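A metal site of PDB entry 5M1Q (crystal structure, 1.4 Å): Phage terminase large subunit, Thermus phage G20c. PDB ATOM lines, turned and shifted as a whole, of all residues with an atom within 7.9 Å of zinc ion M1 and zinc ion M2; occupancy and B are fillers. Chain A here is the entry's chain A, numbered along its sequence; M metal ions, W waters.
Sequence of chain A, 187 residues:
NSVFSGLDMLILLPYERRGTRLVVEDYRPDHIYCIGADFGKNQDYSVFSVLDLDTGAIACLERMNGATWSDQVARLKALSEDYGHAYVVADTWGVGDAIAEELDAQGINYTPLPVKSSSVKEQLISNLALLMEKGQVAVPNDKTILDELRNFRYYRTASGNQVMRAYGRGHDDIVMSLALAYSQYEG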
ATOM      1  N   ALA A  37      10.485  -0.502 -14.229  1.00  0.00           N
ATOM      2  CA  ALA A  37      10.206  -1.949 -14.318  1.00  0.00           C
ATOM      3  C   ALA A  37      11.308  -2.850 -13.762  1.00  0.00           C
ATOM      4  O   ALA A  37      12.456  -2.799 -14.218  1.00  0.00           O
ATOM      5  CB  ALA A  37       9.921  -2.330 -15.759  1.00  0.00           C
ATOM      6  N   ASP A  38      10.939  -3.660 -12.766  1.00  0.00           N
ATOM      7  CA  ASP A  38      11.746  -4.730 -12.181  1.00  0.00           C
ATOM      8  C   ASP A  38      11.117  -6.064 -12.663  1.00  0.00           C
ATOM      9  O   ASP A  38       9.889  -6.103 -12.886  1.00  0.00           O
ATOM     10  CB  ASP A  38      11.682  -4.590 -10.652  1.00  0.00           C
ATOM     11  CG  ASP A  38      12.667  -5.468  -9.931  1.00  0.00           C
ATOM     12  OD1 ASP A  38      13.882  -5.337 -10.157  1.00  0.00           O
ATOM     13  OD2 ASP A  38      12.233  -6.291  -9.097  1.00  0.00           O
ATOM     14  N   PHE A  39      11.938  -7.101 -12.888  1.00  0.00           N
ATOM     15  CA  PHE A  39      11.450  -8.417 -13.374  1.00  0.00           C
ATOM     16  C   PHE A  39      11.846  -9.505 -12.403  1.00  0.00           C
ATOM     17  O   PHE A  39      12.964  -9.469 -11.861  1.00  0.00           O
ATOM     18  CB  PHE A  39      12.056  -8.729 -14.744  1.00  0.00           C
ATOM     19  CG  PHE A  39      11.750  -7.683 -15.780  1.00  0.00           C
ATOM     20  CD1 PHE A  39      10.522  -7.647 -16.407  1.00  0.00           C
ATOM     21  CD2 PHE A  39      12.687  -6.723 -16.100  1.00  0.00           C
ATOM     22  CE1 PHE A  39      10.234  -6.676 -17.353  1.00  0.00           C
ATOM     23  CE2 PHE A  39      12.402  -5.734 -17.030  1.00  0.00           C
ATOM     24  CZ  PHE A  39      11.170  -5.712 -17.661  1.00  0.00           C
ATOM     25  N   GLY A  40      10.948 -10.470 -12.197  1.00  0.00           N
ATOM     26  CA  GLY A  40      11.194 -11.588 -11.279  1.00  0.00           C
ATOM     27  C   GLY A  40      11.528 -12.868 -12.038  1.00  0.00           C
ATOM     28  O   GLY A  40      10.999 -13.087 -13.137  1.00  0.00           O
ATOM     29  N   GLN A  43       8.467 -17.456  -8.681  1.00  0.00           N
ATOM     30  CA  GLN A  43       7.684 -17.040  -7.529  1.00  0.00           C
ATOM     31  C   GLN A  43       8.121 -15.639  -7.041  1.00  0.00           C
ATOM     32  O   GLN A  43       7.467 -15.055  -6.190  1.00  0.00           O
ATOM     33  CB  GLN A  43       7.754 -18.069  -6.393  1.00  0.00           C
ATOM     34  CG  GLN A  43       6.996 -19.360  -6.711  1.00  0.00           C
ATOM     35  CD  GLN A  43       5.482 -19.213  -6.635  1.00  0.00           C
ATOM     36  OE1 GLN A  43       4.777 -19.509  -7.608  1.00  0.00           O
ATOM     37  NE2 GLN A  43       4.986 -18.748  -5.487  1.00  0.00           N
ATOM     38  N   ASP A  44       9.245 -15.134  -7.571  1.00  0.00           N
ATOM     39  CA  ASP A  44       9.648 -13.731  -7.314  1.00  0.00           C
ATOM     40  C   ASP A  44       8.774 -12.800  -8.139  1.00  0.00           C
ATOM     41  O   ASP A  44       8.234 -13.187  -9.195  1.00  0.00           O
ATOM     42  CB  ASP A  44      11.138 -13.488  -7.630  1.00  0.00           C
ATOM     43  CG  ASP A  44      11.699 -12.270  -6.880  1.00  0.00           C
ATOM     44  OD1 ASP A  44      10.998 -11.776  -5.980  1.00  0.00           O
ATOM     45  OD2 ASP A  44      12.837 -11.832  -7.172  1.00  0.00           O
ATOM     46  N   TYR A  45       8.639 -11.561  -7.666  1.00  0.00           N
ATOM     47  CA  TYR A  45       7.702 -10.606  -8.242  1.00  0.00           C
ATOM     48  C   TYR A  45       8.324  -9.696  -9.279  1.00  0.00           C
ATOM     49  O   TYR A  45       9.465  -9.236  -9.133  1.00  0.00           O
ATOM     50  CB  TYR A  45       7.107  -9.736  -7.152  1.00  0.00           C
ATOM     51  CG  TYR A  45       6.194 -10.514  -6.243  1.00  0.00           C
ATOM     52  CD1 TYR A  45       6.712 -11.246  -5.171  1.00  0.00           C
ATOM     53  CD2 TYR A  45       4.815 -10.535  -6.468  1.00  0.00           C
ATOM     54  CE1 TYR A  45       5.861 -11.983  -4.344  1.00  0.00           C
ATOM     55  CE2 TYR A  45       3.969 -11.264  -5.651  1.00  0.00           C
ATOM     56  CZ  TYR A  45       4.501 -11.983  -4.590  1.00  0.00           C
ATOM     57  OH  TYR A  45       3.665 -12.706  -3.774  1.00  0.00           O
ATOM     58  N   SER A  46       7.525  -9.423 -10.307  1.00  0.00           N
ATOM     59  CA  SER A  46       7.788  -8.329 -11.213  1.00  0.00           C
ATOM     60  C   SER A  46       6.922  -7.150 -10.802  1.00  0.00           C
ATOM     61  O   SER A  46       5.761  -7.326 -10.409  1.00  0.00           O
ATOM     62  CB  SER A  46       7.475  -8.737 -12.633  1.00  0.00           C
ATOM     63  OG  SER A  46       8.235  -9.883 -12.956  1.00  0.00           O
ATOM     64  N   VAL A  47       7.482  -5.941 -10.896  1.00  0.00           N
ATOM     65  CA  VAL A  47       6.730  -4.741 -10.501  1.00  0.00           C
ATOM     66  C   VAL A  47       6.957  -3.620 -11.497  1.00  0.00           C
ATOM     67  O   VAL A  47       8.100  -3.269 -11.810  1.00  0.00           O
ATOM     68  CB  VAL A  47       7.130  -4.265  -9.094  1.00  0.00           C
ATOM     69  CG1 VAL A  47       6.321  -3.030  -8.703  1.00  0.00           C
ATOM     70  CG2 VAL A  47       7.025  -5.388  -8.060  1.00  0.00           C
ATOM     71  N   ARG A  63       1.847  -5.377  -9.981  1.00  0.00           N
ATOM     72  CA  ARG A  63       2.730  -6.331  -9.344  1.00  0.00           C
ATOM     73  C   ARG A  63       2.168  -7.733  -9.529  1.00  0.00           C
ATOM     74  O   ARG A  63       0.984  -7.936  -9.326  1.00  0.00           O
ATOM     75  CB  ARG A  63       2.878  -6.026  -7.855  1.00  0.00           C
ATOM     76  CG  ARG A  63       3.707  -7.023  -7.073  1.00  0.00           C
ATOM     77  CD  ARG A  63       3.995  -6.464  -5.701  1.00  0.00           C
ATOM     78  NE  ARG A  63       4.816  -7.323  -4.856  1.00  0.00           N
ATOM     79  CZ  ARG A  63       4.380  -8.214  -3.968  1.00  0.00           C
ATOM     80  NH1 ARG A  63       3.082  -8.444  -3.785  1.00  0.00           N
ATOM     81  NH2 ARG A  63       5.273  -8.902  -3.250  1.00  0.00           N
ATOM     82  N   ASP A  91      15.171  -2.469 -15.597  1.00  0.00           N
ATOM     83  CA  ASP A  91      16.327  -3.220 -15.125  1.00  0.00           C
ATOM     84  C   ASP A  91      16.508  -4.447 -16.051  1.00  0.00           C
ATOM     85  O   ASP A  91      15.890  -5.488 -15.857  1.00  0.00           O
ATOM     86  CB  ASP A  91      16.143  -3.649 -13.675  1.00  0.00           C
ATOM     87  CG  ASP A  91      17.342  -4.424 -13.137  1.00  0.00           C
ATOM     88  OD1 ASP A  91      18.377  -4.493 -13.844  1.00  0.00           O
ATOM     89  OD2 ASP A  91      17.227  -4.980 -12.040  1.00  0.00           O
ATOM     90  N   GLU A 148       7.410  -3.189   2.336  1.00  0.00           N
ATOM     91  CA  GLU A 148       8.685  -3.269   1.618  1.00  0.00           C
ATOM     92  C   GLU A 148       9.540  -2.052   1.868  1.00  0.00           C
ATOM     93  O   GLU A 148      10.734  -2.177   2.031  1.00  0.00           O
ATOM     94  CB  GLU A 148       8.497  -3.437   0.090  1.00  0.00           C
ATOM     95  CG  GLU A 148       7.995  -4.816  -0.315  1.00  0.00           C
ATOM     96  CD  GLU A 148       8.449  -5.320  -1.674  1.00  0.00           C
ATOM     97  OE1 GLU A 148       9.287  -4.696  -2.371  1.00  0.00           O
ATOM     98  OE2 GLU A 148       7.947  -6.384  -2.055  1.00  0.00           O
ATOM     99  N   GLY A 170      12.286 -11.622   2.081  1.00  0.00           N
ATOM    100  CA  GLY A 170      12.333 -10.183   2.272  1.00  0.00           C
ATOM    101  C   GLY A 170      12.488  -9.436   0.954  1.00  0.00           C
ATOM    102  O   GLY A 170      13.585  -8.993   0.610  1.00  0.00           O
ATOM    103  N   HIS A 171      11.379  -9.299   0.238  1.00  0.00           N
ATOM    104  CA  HIS A 171      11.382  -8.753  -1.126  1.00  0.00           C
ATOM    105  C   HIS A 171      11.650  -7.248  -1.157  1.00  0.00           C
ATOM    106  O   HIS A 171      11.246  -6.524  -0.232  1.00  0.00           O
ATOM    107  CB  HIS A 171      10.025  -8.974  -1.784  1.00  0.00           C
ATOM    108  CG  HIS A 171       9.690 -10.409  -2.028  1.00  0.00           C
ATOM    109  ND1 HIS A 171      10.365 -11.192  -2.935  1.00  0.00           N
ATOM    110  CD2 HIS A 171       8.697 -11.192  -1.527  1.00  0.00           C
ATOM    111  CE1 HIS A 171       9.846 -12.406  -2.955  1.00  0.00           C
ATOM    112  NE2 HIS A 171       8.835 -12.433  -2.113  1.00  0.00           N
ATOM    113  N   ASP A 172      12.309  -6.809  -2.219  1.00  0.00           N
ATOM    114  CA  ASP A 172      12.523  -5.367  -2.499  1.00  0.00           C
ATOM    115  C   ASP A 172      12.138  -4.986  -3.936  1.00  0.00           C
ATOM    116  O   ASP A 172      12.515  -3.918  -4.411  1.00  0.00           O
ATOM    117  CB  ASP A 172      13.980  -4.981  -2.212  1.00  0.00           C
ATOM    118  CG  ASP A 172      14.972  -5.513  -3.259  1.00  0.00           C
ATOM    119  OD1 ASP A 172      14.617  -6.351  -4.124  1.00  0.00           O
ATOM    120  OD2 ASP A 172      16.139  -5.071  -3.216  1.00  0.00           O
ATOM    121  N   ASP A 173      11.347  -5.812  -4.619  1.00  0.00           N
ATOM    122  CA  ASP A 173      10.981  -5.549  -6.004  1.00  0.00           C
ATOM    123  C   ASP A 173      10.142  -4.254  -6.190  1.00  0.00           C
ATOM    124  O   ASP A 173      10.294  -3.551  -7.190  1.00  0.00           O
ATOM    125  CB  ASP A 173      10.196  -6.704  -6.607  1.00  0.00           C
ATOM    126  CG  ASP A 173      10.764  -8.027  -6.226  1.00  0.00           C
ATOM    127  OD1 ASP A 173      11.808  -8.401  -6.802  1.00  0.00           O
ATOM    128  OD2 ASP A 173      10.203  -8.625  -5.284  1.00  0.00           O
ATOM    129  N   ILE A 174       9.277  -3.962  -5.223  1.00  0.00           N
ATOM    130  CA  ILE A 174       8.494  -2.717  -5.256  1.00  0.00           C
ATOM    131  C   ILE A 174       9.417  -1.524  -5.080  1.00  0.00           C
ATOM    132  O   ILE A 174       9.301  -0.557  -5.837  1.00  0.00           O
ATOM    133  CB  ILE A 174       7.384  -2.681  -4.184  1.00  0.00           C
ATOM    134  CG1 ILE A 174       6.378  -3.808  -4.455  1.00  0.00           C
ATOM    135  CG2 ILE A 174       6.678  -1.340  -4.151  1.00  0.00           C
ATOM    136  CD1 ILE A 174       5.493  -4.108  -3.274  1.00  0.00           C
ATOM    137  N   MET A 176      12.608  -1.277  -5.772  1.00  0.00           N
ATOM    138  CA  MET A 176      13.412  -1.079  -6.965  1.00  0.00           C
ATOM    139  C   MET A 176      12.622  -0.490  -8.126  1.00  0.00           C
ATOM    140  O   MET A 176      13.098   0.379  -8.835  1.00  0.00           O
ATOM    141  CB  MET A 176      14.124  -2.366  -7.357  1.00  0.00           C
ATOM    142  CG  MET A 176      15.152  -2.804  -6.325  1.00  0.00           C
ATOM    143  SD  MET A 176      16.370  -1.522  -5.909  1.00  0.00           S
ATOM    144  CE  MET A 176      17.000  -1.077  -7.514  1.00  0.00           C
ATOM    145  N   SER A 177      11.391  -0.965  -8.316  1.00  0.00           N
ATOM    146  CA  SER A 177      10.554  -0.416  -9.356  1.00  0.00           C
ATOM    147  C   SER A 177      10.252   1.079  -9.137  1.00  0.00           C
ATOM    148  O   SER A 177      10.342   1.899 -10.044  1.00  0.00           O
ATOM    149  CB  SER A 177       9.257  -1.205  -9.405  1.00  0.00           C
ATOM    150  OG  SER A 177       8.347  -0.633 -10.303  1.00  0.00           O
HETATM  151 ZN    ZN M   1      11.338 -10.286  -4.667  1.00  0.00          ZN
HETATM  152 ZN    ZN M   2      13.266  -7.901  -8.088  1.00  0.00          ZN
HETATM  153  O   HOH W   1      12.070  -8.755  -9.408  1.00  0.00           O
HETATM  154  O   HOH W   2      13.312  -9.606  -3.958  1.00  0.00           O
HETATM  155  O   HOH W   3      14.610  -7.948  -9.512  1.00  0.00           O
HETATM  156  O   HOH W   4      14.301  -6.603  -6.869  1.00  0.00           O
HETATM  157  O   HOH W   5      14.284  -9.633  -7.030  1.00  0.00           O
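Zinc ion M1 is bound by the side-chain carboxylate of Asp 44, the side-chain carboxylate of Asp 173, a ring nitrogen (ND1) of His 171 and water W2.
Water W3 lies within hydrogen-bond range of OD1 of Asp 38 and O of Phe 39.
Water W1 lies within hydrogen-bond range of the backbone carbonyl oxygen (O) of Tyr 45, the backbone carbonyl oxygen (O) of Phe 39 and the backbone NH (N) of Gly 40.
The backbone NH (N) of Asp 173 is in hydrogen-bond range of the side-chain carboxylate (OE1) of Glu 148, at 3.2 Å.
N of Asp 38 sits at hydrogen-bond distance from O of Val 47.
Water W3 binds zinc ion M2, at 2.0 Å.
Water W1 is bound to zinc ion M2 (2.0 Å).
Zinc ion M2 is bound by the side-chain carboxylate (OD1) of Asp 173 (2.0 Å).
Zinc ion M2 is bound by water W4, at 2.1 Å.
OD2 of Asp 38 binds zinc ion M2 (2.2 Å).
Water W5 binds zinc ion M2 (2.3 Å).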
